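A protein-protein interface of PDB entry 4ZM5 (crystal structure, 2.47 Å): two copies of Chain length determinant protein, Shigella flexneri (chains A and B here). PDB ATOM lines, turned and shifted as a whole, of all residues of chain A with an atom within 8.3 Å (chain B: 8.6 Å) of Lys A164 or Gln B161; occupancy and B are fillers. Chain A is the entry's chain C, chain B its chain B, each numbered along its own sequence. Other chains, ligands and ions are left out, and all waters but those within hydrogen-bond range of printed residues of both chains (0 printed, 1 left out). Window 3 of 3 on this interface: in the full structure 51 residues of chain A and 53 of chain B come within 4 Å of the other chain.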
ATOM      1  N   ALA A 157      -0.987   0.069 -21.848  1.00  0.00           N
ATOM      2  CA  ALA A 157      -0.330  -0.972 -22.655  1.00  0.00           C
ATOM      3  C   ALA A 157       0.235  -0.366 -23.928  1.00  0.00           C
ATOM      4  O   ALA A 157       1.349  -0.721 -24.320  1.00  0.00           O
ATOM      5  CB  ALA A 157      -1.302  -2.108 -22.983  1.00  0.00           C
ATOM      6  N   GLN A 161       4.097   0.087 -24.707  1.00  0.00           N
ATOM      7  CA  GLN A 161       4.373  -0.827 -25.824  1.00  0.00           C
ATOM      8  C   GLN A 161       4.372  -2.294 -25.336  1.00  0.00           C
ATOM      9  O   GLN A 161       5.269  -3.062 -25.676  1.00  0.00           O
ATOM     10  CB  GLN A 161       5.690  -0.482 -26.555  1.00  0.00           C
ATOM     11  CG  GLN A 161       5.829   0.964 -26.975  1.00  0.00           C
ATOM     12  CD  GLN A 161       7.032   1.219 -27.857  1.00  0.00           C
ATOM     13  OE1 GLN A 161       6.901   1.500 -29.052  1.00  0.00           O
ATOM     14  NE2 GLN A 161       8.231   1.167 -27.293  1.00  0.00           N
ATOM     15  N   VAL A 162       3.357  -2.663 -24.522  1.00  0.00           N
ATOM     16  CA  VAL A 162       3.100  -4.011 -23.986  1.00  0.00           C
ATOM     17  C   VAL A 162       2.020  -4.585 -24.919  1.00  0.00           C
ATOM     18  O   VAL A 162       0.845  -4.273 -24.753  1.00  0.00           O
ATOM     19  CB  VAL A 162       2.679  -3.947 -22.474  1.00  0.00           C
ATOM     20  CG1 VAL A 162       2.407  -5.331 -21.893  1.00  0.00           C
ATOM     21  CG2 VAL A 162       3.723  -3.229 -21.635  1.00  0.00           C
ATOM     22  N   THR A 163       2.425  -5.321 -25.971  1.00  0.00           N
ATOM     23  CA  THR A 163       1.489  -5.813 -27.002  1.00  0.00           C
ATOM     24  C   THR A 163       1.021  -7.248 -26.702  1.00  0.00           C
ATOM     25  O   THR A 163      -0.174  -7.563 -26.793  1.00  0.00           O
ATOM     26  CB  THR A 163       2.143  -5.681 -28.386  1.00  0.00           C
ATOM     27  OG1 THR A 163       2.653  -4.350 -28.522  1.00  0.00           O
ATOM     28  CG2 THR A 163       1.175  -5.947 -29.524  1.00  0.00           C
ATOM     29  N   LYS A 164       1.966  -8.103 -26.329  1.00  0.00           N
ATOM     30  CA  LYS A 164       1.712  -9.497 -25.969  1.00  0.00           C
ATOM     31  C   LYS A 164       1.603  -9.596 -24.439  1.00  0.00           C
ATOM     32  O   LYS A 164       2.094  -8.697 -23.750  1.00  0.00           O
ATOM     33  CB  LYS A 164       2.835 -10.403 -26.527  1.00  0.00           C
ATOM     34  CG  LYS A 164       2.999 -10.333 -28.052  1.00  0.00           C
ATOM     35  CD  LYS A 164       2.094 -11.322 -28.782  1.00  0.00           C
ATOM     36  CE  LYS A 164       2.068 -11.063 -30.261  1.00  0.00           C
ATOM     37  NZ  LYS A 164       1.181 -12.019 -30.962  1.00  0.00           N
ATOM     38  N   PRO A 165       0.941 -10.641 -23.873  1.00  0.00           N
ATOM     39  CA  PRO A 165       0.884 -10.745 -22.410  1.00  0.00           C
ATOM     40  C   PRO A 165       2.268 -10.807 -21.756  1.00  0.00           C
ATOM     41  O   PRO A 165       3.188 -11.384 -22.326  1.00  0.00           O
ATOM     42  CB  PRO A 165       0.139 -12.058 -22.176  1.00  0.00           C
ATOM     43  CG  PRO A 165      -0.473 -12.410 -23.448  1.00  0.00           C
ATOM     44  CD  PRO A 165       0.286 -11.796 -24.527  1.00  0.00           C
ATOM     45  N   GLN A 166       2.409 -10.205 -20.567  1.00  0.00           N
ATOM     46  CA  GLN A 166       3.631 -10.259 -19.766  1.00  0.00           C
ATOM     47  C   GLN A 166       3.246 -10.741 -18.358  1.00  0.00           C
ATOM     48  O   GLN A 166       3.471 -10.051 -17.353  1.00  0.00           O
ATOM     49  CB  GLN A 166       4.386  -8.927 -19.748  1.00  0.00           C
ATOM     50  CG  GLN A 166       5.829  -9.093 -19.249  1.00  0.00           C
ATOM     51  CD  GLN A 166       6.639  -7.813 -19.240  1.00  0.00           C
ATOM     52  OE1 GLN A 166       6.261  -6.782 -19.829  1.00  0.00           O
ATOM     53  NE2 GLN A 166       7.788  -7.865 -18.569  1.00  0.00           N
ATOM     54  N   VAL A 167       2.647 -11.952 -18.314  1.00  0.00           N
ATOM     55  CA  VAL A 167       2.193 -12.606 -17.092  1.00  0.00           C
ATOM     56  C   VAL A 167       3.028 -13.861 -16.851  1.00  0.00           C
ATOM     57  O   VAL A 167       3.163 -14.697 -17.750  1.00  0.00           O
ATOM     58  CB  VAL A 167       0.675 -12.931 -17.137  1.00  0.00           C
ATOM     59  CG1 VAL A 167       0.181 -13.416 -15.791  1.00  0.00           C
ATOM     60  CG2 VAL A 167      -0.142 -11.725 -17.606  1.00  0.00           C
ATOM     61  N   PHE A 179      -3.054  -4.181 -17.736  1.00  0.00           N
ATOM     62  CA  PHE A 179      -2.220  -3.838 -18.907  1.00  0.00           C
ATOM     63  C   PHE A 179      -1.181  -4.903 -19.174  1.00  0.00           C
ATOM     64  O   PHE A 179      -0.696  -4.990 -20.305  1.00  0.00           O
ATOM     65  CB  PHE A 179      -1.541  -2.469 -18.778  1.00  0.00           C
ATOM     66  CG  PHE A 179      -0.942  -2.232 -17.419  1.00  0.00           C
ATOM     67  CD1 PHE A 179      -1.599  -1.447 -16.484  1.00  0.00           C
ATOM     68  CD2 PHE A 179       0.286  -2.796 -17.072  1.00  0.00           C
ATOM     69  CE1 PHE A 179      -1.049  -1.233 -15.236  1.00  0.00           C
ATOM     70  CE2 PHE A 179       0.816  -2.609 -15.802  1.00  0.00           C
ATOM     71  CZ  PHE A 179       0.145  -1.824 -14.897  1.00  0.00           C
ATOM     72  N   LEU A 180      -0.887  -5.751 -18.155  1.00  0.00           N
ATOM     73  CA  LEU A 180       0.047  -6.871 -18.261  1.00  0.00           C
ATOM     74  C   LEU A 180      -0.444  -7.916 -19.258  1.00  0.00           C
ATOM     75  O   LEU A 180       0.344  -8.740 -19.693  1.00  0.00           O
ATOM     76  CB  LEU A 180       0.267  -7.539 -16.885  1.00  0.00           C
ATOM     77  CG  LEU A 180       1.115  -6.800 -15.878  1.00  0.00           C
ATOM     78  CD1 LEU A 180       0.882  -7.373 -14.503  1.00  0.00           C
ATOM     79  CD2 LEU A 180       2.585  -6.929 -16.214  1.00  0.00           C
ATOM     80  N   LEU A 181      -1.742  -7.898 -19.600  1.00  0.00           N
ATOM     81  CA  LEU A 181      -2.347  -8.831 -20.550  1.00  0.00           C
ATOM     82  C   LEU A 181      -1.997  -8.475 -22.001  1.00  0.00           C
ATOM     83  O   LEU A 181      -2.161  -9.319 -22.883  1.00  0.00           O
ATOM     84  CB  LEU A 181      -3.869  -8.875 -20.349  1.00  0.00           C
ATOM     85  CG  LEU A 181      -4.338  -9.364 -18.958  1.00  0.00           C
ATOM     86  CD1 LEU A 181      -5.834  -9.299 -18.851  1.00  0.00           C
ATOM     87  CD2 LEU A 181      -3.867 -10.771 -18.671  1.00  0.00           C
ATOM     88  N   GLY A 182      -1.484  -7.261 -22.224  1.00  0.00           N
ATOM     89  CA  GLY A 182      -1.066  -6.775 -23.536  1.00  0.00           C
ATOM     90  C   GLY A 182      -2.175  -6.080 -24.292  1.00  0.00           C
ATOM     91  O   GLY A 182      -3.339  -6.438 -24.127  1.00  0.00           O
ATOM     92  N   SER A 183      -1.823  -5.087 -25.134  1.00  0.00           N
ATOM     93  CA  SER A 183      -2.796  -4.304 -25.908  1.00  0.00           C
ATOM     94  C   SER A 183      -3.663  -5.160 -26.858  1.00  0.00           C
ATOM     95  O   SER A 183      -4.836  -4.839 -27.050  1.00  0.00           O
ATOM     96  CB  SER A 183      -2.094  -3.202 -26.695  1.00  0.00           C
ATOM     97  OG  SER A 183      -1.146  -3.704 -27.622  1.00  0.00           O
ATOM     98  N   GLU A 184      -3.098  -6.243 -27.414  1.00  0.00           N
ATOM     99  CA  GLU A 184      -3.781  -7.121 -28.355  1.00  0.00           C
ATOM    100  C   GLU A 184      -5.001  -7.818 -27.726  1.00  0.00           C
ATOM    101  O   GLU A 184      -6.099  -7.775 -28.299  1.00  0.00           O
ATOM    102  CB  GLU A 184      -2.807  -8.164 -28.920  1.00  0.00           C
ATOM    103  CG  GLU A 184      -2.323  -7.880 -30.327  1.00  0.00           C
ATOM    104  CD  GLU A 184      -1.278  -8.869 -30.802  1.00  0.00           C
ATOM    105  OE1 GLU A 184      -1.544  -9.589 -31.794  1.00  0.00           O
ATOM    106  OE2 GLU A 184      -0.209  -8.956 -30.159  1.00  0.00           O
ATOM    107  N   ALA A 185      -4.821  -8.449 -26.567  1.00  0.00           N
ATOM    108  CA  ALA A 185      -5.926  -9.117 -25.891  1.00  0.00           C
ATOM    109  C   ALA A 185      -6.881  -8.087 -25.313  1.00  0.00           C
ATOM    110  O   ALA A 185      -8.091  -8.303 -25.405  1.00  0.00           O
ATOM    111  CB  ALA A 185      -5.415 -10.042 -24.810  1.00  0.00           C
ATOM    112  N   LEU B 154     -11.330 -17.485 -25.811  1.00  0.00           N
ATOM    113  CA  LEU B 154     -10.768 -18.058 -27.032  1.00  0.00           C
ATOM    114  C   LEU B 154     -10.679 -16.981 -28.112  1.00  0.00           C
ATOM    115  O   LEU B 154      -9.723 -16.984 -28.887  1.00  0.00           O
ATOM    116  CB  LEU B 154     -11.605 -19.264 -27.497  1.00  0.00           C
ATOM    117  CG  LEU B 154     -11.239 -19.919 -28.845  1.00  0.00           C
ATOM    118  CD1 LEU B 154      -9.838 -20.491 -28.826  1.00  0.00           C
ATOM    119  CD2 LEU B 154     -12.186 -20.996 -29.159  1.00  0.00           C
ATOM    120  N   GLN B 155     -11.642 -16.030 -28.135  1.00  0.00           N
ATOM    121  CA  GLN B 155     -11.599 -14.915 -29.099  1.00  0.00           C
ATOM    122  C   GLN B 155     -10.390 -14.008 -28.783  1.00  0.00           C
ATOM    123  O   GLN B 155      -9.690 -13.597 -29.710  1.00  0.00           O
ATOM    124  CB  GLN B 155     -12.902 -14.099 -29.079  1.00  0.00           C
ATOM    125  CG  GLN B 155     -14.152 -14.876 -29.487  1.00  0.00           C
ATOM    126  CD  GLN B 155     -15.436 -14.073 -29.291  1.00  0.00           C
ATOM    127  OE1 GLN B 155     -15.675 -13.465 -28.240  1.00  0.00           O
ATOM    128  NE2 GLN B 155     -16.312 -14.082 -30.287  1.00  0.00           N
ATOM    129  N   TYR B 156     -10.107 -13.759 -27.457  1.00  0.00           N
ATOM    130  CA  TYR B 156      -8.972 -12.937 -27.015  1.00  0.00           C
ATOM    131  C   TYR B 156      -7.632 -13.629 -27.334  1.00  0.00           C
ATOM    132  O   TYR B 156      -6.672 -12.961 -27.754  1.00  0.00           O
ATOM    133  CB  TYR B 156      -9.023 -12.590 -25.498  1.00  0.00           C
ATOM    134  CG  TYR B 156     -10.363 -12.241 -24.888  1.00  0.00           C
ATOM    135  CD1 TYR B 156     -11.336 -11.561 -25.620  1.00  0.00           C
ATOM    136  CD2 TYR B 156     -10.620 -12.489 -23.539  1.00  0.00           C
ATOM    137  CE1 TYR B 156     -12.563 -11.226 -25.055  1.00  0.00           C
ATOM    138  CE2 TYR B 156     -11.840 -12.148 -22.961  1.00  0.00           C
ATOM    139  CZ  TYR B 156     -12.808 -11.514 -23.723  1.00  0.00           C
ATOM    140  OH  TYR B 156     -14.002 -11.171 -23.149  1.00  0.00           O
ATOM    141  N   ALA B 157      -7.561 -14.966 -27.088  1.00  0.00           N
ATOM    142  CA  ALA B 157      -6.364 -15.782 -27.331  1.00  0.00           C
ATOM    143  C   ALA B 157      -6.007 -15.786 -28.813  1.00  0.00           C
ATOM    144  O   ALA B 157      -4.830 -15.702 -29.153  1.00  0.00           O
ATOM    145  CB  ALA B 157      -6.583 -17.204 -26.840  1.00  0.00           C
ATOM    146  N   ASN B 158      -7.024 -15.836 -29.693  1.00  0.00           N
ATOM    147  CA  ASN B 158      -6.820 -15.806 -31.140  1.00  0.00           C
ATOM    148  C   ASN B 158      -6.367 -14.429 -31.614  1.00  0.00           C
ATOM    149  O   ASN B 158      -5.541 -14.365 -32.512  1.00  0.00           O
ATOM    150  CB  ASN B 158      -8.097 -16.216 -31.884  1.00  0.00           C
ATOM    151  CG  ASN B 158      -8.418 -17.691 -31.834  1.00  0.00           C
ATOM    152  OD1 ASN B 158      -7.546 -18.562 -31.682  1.00  0.00           O
ATOM    153  ND2 ASN B 158      -9.677 -18.007 -32.042  1.00  0.00           N
ATOM    154  N   GLN B 159      -6.914 -13.328 -31.047  1.00  0.00           N
ATOM    155  CA  GLN B 159      -6.512 -11.981 -31.480  1.00  0.00           C
ATOM    156  C   GLN B 159      -5.086 -11.663 -31.020  1.00  0.00           C
ATOM    157  O   GLN B 159      -4.325 -11.048 -31.776  1.00  0.00           O
ATOM    158  CB  GLN B 159      -7.483 -10.885 -31.021  1.00  0.00           C
ATOM    159  CG  GLN B 159      -7.564  -9.735 -32.047  1.00  0.00           C
ATOM    160  CD  GLN B 159      -8.232  -8.476 -31.516  1.00  0.00           C
ATOM    161  OE1 GLN B 159      -9.479  -8.372 -31.458  1.00  0.00           O
ATOM    162  NE2 GLN B 159      -7.410  -7.469 -31.161  1.00  0.00           N
ATOM    163  N   ALA B 160      -4.725 -12.102 -29.798  1.00  0.00           N
ATOM    164  CA  ALA B 160      -3.390 -11.916 -29.235  1.00  0.00           C
ATOM    165  C   ALA B 160      -2.398 -12.925 -29.827  1.00  0.00           C
ATOM    166  O   ALA B 160      -1.203 -12.824 -29.554  1.00  0.00           O
ATOM    167  CB  ALA B 160      -3.436 -12.049 -27.721  1.00  0.00           C
ATOM    168  N   GLN B 161      -2.901 -13.882 -30.645  1.00  0.00           N
ATOM    169  CA  GLN B 161      -2.173 -14.946 -31.345  1.00  0.00           C
ATOM    170  C   GLN B 161      -1.387 -15.852 -30.368  1.00  0.00           C
ATOM    171  O   GLN B 161      -0.312 -16.360 -30.715  1.00  0.00           O
ATOM    172  CB  GLN B 161      -1.249 -14.364 -32.422  1.00  0.00           C
ATOM    173  CG  GLN B 161      -1.983 -13.597 -33.514  1.00  0.00           C
ATOM    174  CD  GLN B 161      -1.379 -13.878 -34.856  1.00  0.00           C
ATOM    175  OE1 GLN B 161      -0.252 -13.465 -35.152  1.00  0.00           O
ATOM    176  NE2 GLN B 161      -2.110 -14.609 -35.693  1.00  0.00           N
ATOM    177  N   VAL B 162      -1.955 -16.085 -29.160  1.00  0.00           N
ATOM    178  CA  VAL B 162      -1.342 -16.942 -28.132  1.00  0.00           C
ATOM    179  C   VAL B 162      -2.014 -18.342 -28.159  1.00  0.00           C
ATOM    180  O   VAL B 162      -3.190 -18.477 -27.831  1.00  0.00           O
ATOM    181  CB  VAL B 162      -1.303 -16.299 -26.709  1.00  0.00           C
ATOM    182  CG1 VAL B 162      -0.287 -15.155 -26.666  1.00  0.00           C
ATOM    183  CG2 VAL B 162      -2.670 -15.827 -26.241  1.00  0.00           C
ATOM    184  N   THR B 163      -1.261 -19.366 -28.616  1.00  0.00           N
ATOM    185  CA  THR B 163      -1.773 -20.732 -28.790  1.00  0.00           C
ATOM    186  C   THR B 163      -1.399 -21.654 -27.634  1.00  0.00           C
ATOM    187  O   THR B 163      -2.172 -22.543 -27.284  1.00  0.00           O
ATOM    188  CB  THR B 163      -1.255 -21.327 -30.096  1.00  0.00           C
ATOM    189  OG1 THR B 163       0.168 -21.274 -30.074  1.00  0.00           O
ATOM    190  CG2 THR B 163      -1.792 -20.622 -31.323  1.00  0.00           C
ATOM    191  N   LYS B 164      -0.190 -21.478 -27.079  1.00  0.00           N
ATOM    192  CA  LYS B 164       0.298 -22.300 -25.980  1.00  0.00           C
ATOM    193  C   LYS B 164       0.065 -21.556 -24.668  1.00  0.00           C
ATOM    194  O   LYS B 164      -0.098 -20.333 -24.705  1.00  0.00           O
ATOM    195  CB  LYS B 164       1.792 -22.638 -26.195  1.00  0.00           C
ATOM    196  CG  LYS B 164       2.057 -23.448 -27.471  1.00  0.00           C
ATOM    197  CD  LYS B 164       2.228 -24.945 -27.167  1.00  0.00           C
ATOM    198  CE  LYS B 164       1.706 -25.919 -28.211  1.00  0.00           C
ATOM    199  NZ  LYS B 164       2.198 -25.648 -29.596  1.00  0.00           N
ATOM    200  N   GLN B 166       0.547 -19.358 -21.385  1.00  0.00           N
ATOM    201  CA  GLN B 166       1.470 -18.240 -21.131  1.00  0.00           C
ATOM    202  C   GLN B 166       1.867 -18.132 -19.674  1.00  0.00           C
ATOM    203  O   GLN B 166       2.621 -17.236 -19.295  1.00  0.00           O
ATOM    204  CB  GLN B 166       0.797 -16.906 -21.548  1.00  0.00           C
ATOM    205  CG  GLN B 166       0.470 -16.779 -23.031  1.00  0.00           C
ATOM    206  CD  GLN B 166       1.707 -16.749 -23.888  1.00  0.00           C
ATOM    207  OE1 GLN B 166       2.560 -15.845 -23.775  1.00  0.00           O
ATOM    208  NE2 GLN B 166       1.819 -17.743 -24.766  1.00  0.00           N
ATOM    209  N   PHE B 179      -7.607 -16.541 -21.268  1.00  0.00           N
ATOM    210  CA  PHE B 179      -6.957 -16.562 -22.590  1.00  0.00           C
ATOM    211  C   PHE B 179      -5.470 -16.955 -22.461  1.00  0.00           C
ATOM    212  O   PHE B 179      -4.872 -17.438 -23.426  1.00  0.00           O
ATOM    213  CB  PHE B 179      -7.128 -15.207 -23.310  1.00  0.00           C
ATOM    214  CG  PHE B 179      -6.056 -14.186 -23.029  1.00  0.00           C
ATOM    215  CD1 PHE B 179      -6.134 -13.360 -21.912  1.00  0.00           C
ATOM    216  CD2 PHE B 179      -4.947 -14.070 -23.861  1.00  0.00           C
ATOM    217  CE1 PHE B 179      -5.130 -12.431 -21.636  1.00  0.00           C
ATOM    218  CE2 PHE B 179      -3.937 -13.146 -23.580  1.00  0.00           C
ATOM    219  CZ  PHE B 179      -4.039 -12.327 -22.472  1.00  0.00           C
ATOM    220  N   LEU B 180      -4.885 -16.750 -21.267  1.00  0.00           N
ATOM    221  CA  LEU B 180      -3.486 -17.079 -20.988  1.00  0.00           C
ATOM    222  C   LEU B 180      -3.231 -18.591 -21.020  1.00  0.00           C
ATOM    223  O   LEU B 180      -2.070 -19.008 -21.005  1.00  0.00           O
ATOM    224  CB  LEU B 180      -3.045 -16.520 -19.645  1.00  0.00           C
ATOM    225  CG  LEU B 180      -2.945 -15.003 -19.513  1.00  0.00           C
ATOM    226  CD1 LEU B 180      -2.765 -14.611 -18.055  1.00  0.00           C
ATOM    227  CD2 LEU B 180      -1.805 -14.436 -20.316  1.00  0.00           C
ATOM    228  N   GLY B 182      -4.087 -20.341 -23.538  1.00  0.00           N
ATOM    229  CA  GLY B 182      -3.796 -20.534 -24.954  1.00  0.00           C
ATOM    230  C   GLY B 182      -5.002 -21.008 -25.713  1.00  0.00           C
ATOM    231  O   GLY B 182      -5.798 -21.760 -25.159  1.00  0.00           O
ATOM    232  N   SER B 183      -5.124 -20.620 -26.995  1.00  0.00           N
ATOM    233  CA  SER B 183      -6.248 -21.010 -27.857  1.00  0.00           C
ATOM    234  C   SER B 183      -6.383 -22.534 -28.014  1.00  0.00           C
ATOM    235  O   SER B 183      -7.507 -23.027 -28.101  1.00  0.00           O
ATOM    236  CB  SER B 183      -6.144 -20.353 -29.227  1.00  0.00           C
ATOM    237  OG  SER B 183      -4.944 -20.716 -29.889  1.00  0.00           O
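NE2 of Gln B159 sits at hydrogen-bond distance from O of Glu A184 (3.2 Å).
O of Ala B160 is in hydrogen-bond range of NZ of Lys A164, at 2.9 Å.
O of Val A167 lies close to O of Gln B166 (3.0 Å).
NE2 of Gln B166 is in hydrogen-bond range of O of Lys B164, at 3.2 Å.
N of Gln B166 lies within hydrogen-bond range of O of Leu B180 (2.7 Å).
The backbone carbonyl oxygen of Thr A163 lies within hydrogen-bond range of the backbone NH of Glu A184 (3.3 Å).
The side-chain carboxylate (OE2) of Glu A184 is in salt-bridge range of the side-chain amino group (NZ) of Lys A164 (3.5 Å).
Among the printed residues, pairs that only touch across the chains: Pro A165 with Phe B179 (3.5 Å), Ala A185 with Phe B179 (3.5 Å), Leu A181 with Phe B179 (3.6 Å), Pro A165 with Leu B180 (3.6 Å), Lys A164 with Gln B161 (3.7 Å), Glu A184 with Ala B160 (3.8 Å) and Val A167 with Leu B180 (3.9 Å).
Lys A164 touches just these residues of chain B: Ala B160 and Gln B161.
Gln B161 touches one residue of chain A.
No residue of chain B comes within 4 Å of Thr A163.
Ala B160 touches just these residues of chain A: Lys A164 and Glu A184.
Printed residues of chain B within 4 Å of Glu A184: Gln B159 and Ala B160.
Printed residues of chain B within 4 Å of Leu A181: Phe B179.
Printed residues of chain A within 4 Å of Phe B179: Pro A165 (3.5 Å), Leu A181 (3.6 Å) and Ala A185 (3.5 Å).
Val A162 touches none of the printed residues of chain B.
Of the 16 printed residues of chain B, 6 touch a printed residue of chain A.
Of the 15 printed residues of chain A, 6 touch a printed residue of chain B.
Hydrophobic or aromatic side chains of chain A that line the printed part of chain B: Pro A165, Val A167, Leu A181 and Ala A185.
Lys A164 touches Gln B161, but with the chains exchanged Gln A161 does not touch Lys B164 (18.1 Å).
Of the 10 pairs that touch across the chains among the printed residues, none has its exchanged pair printed and touching as well.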
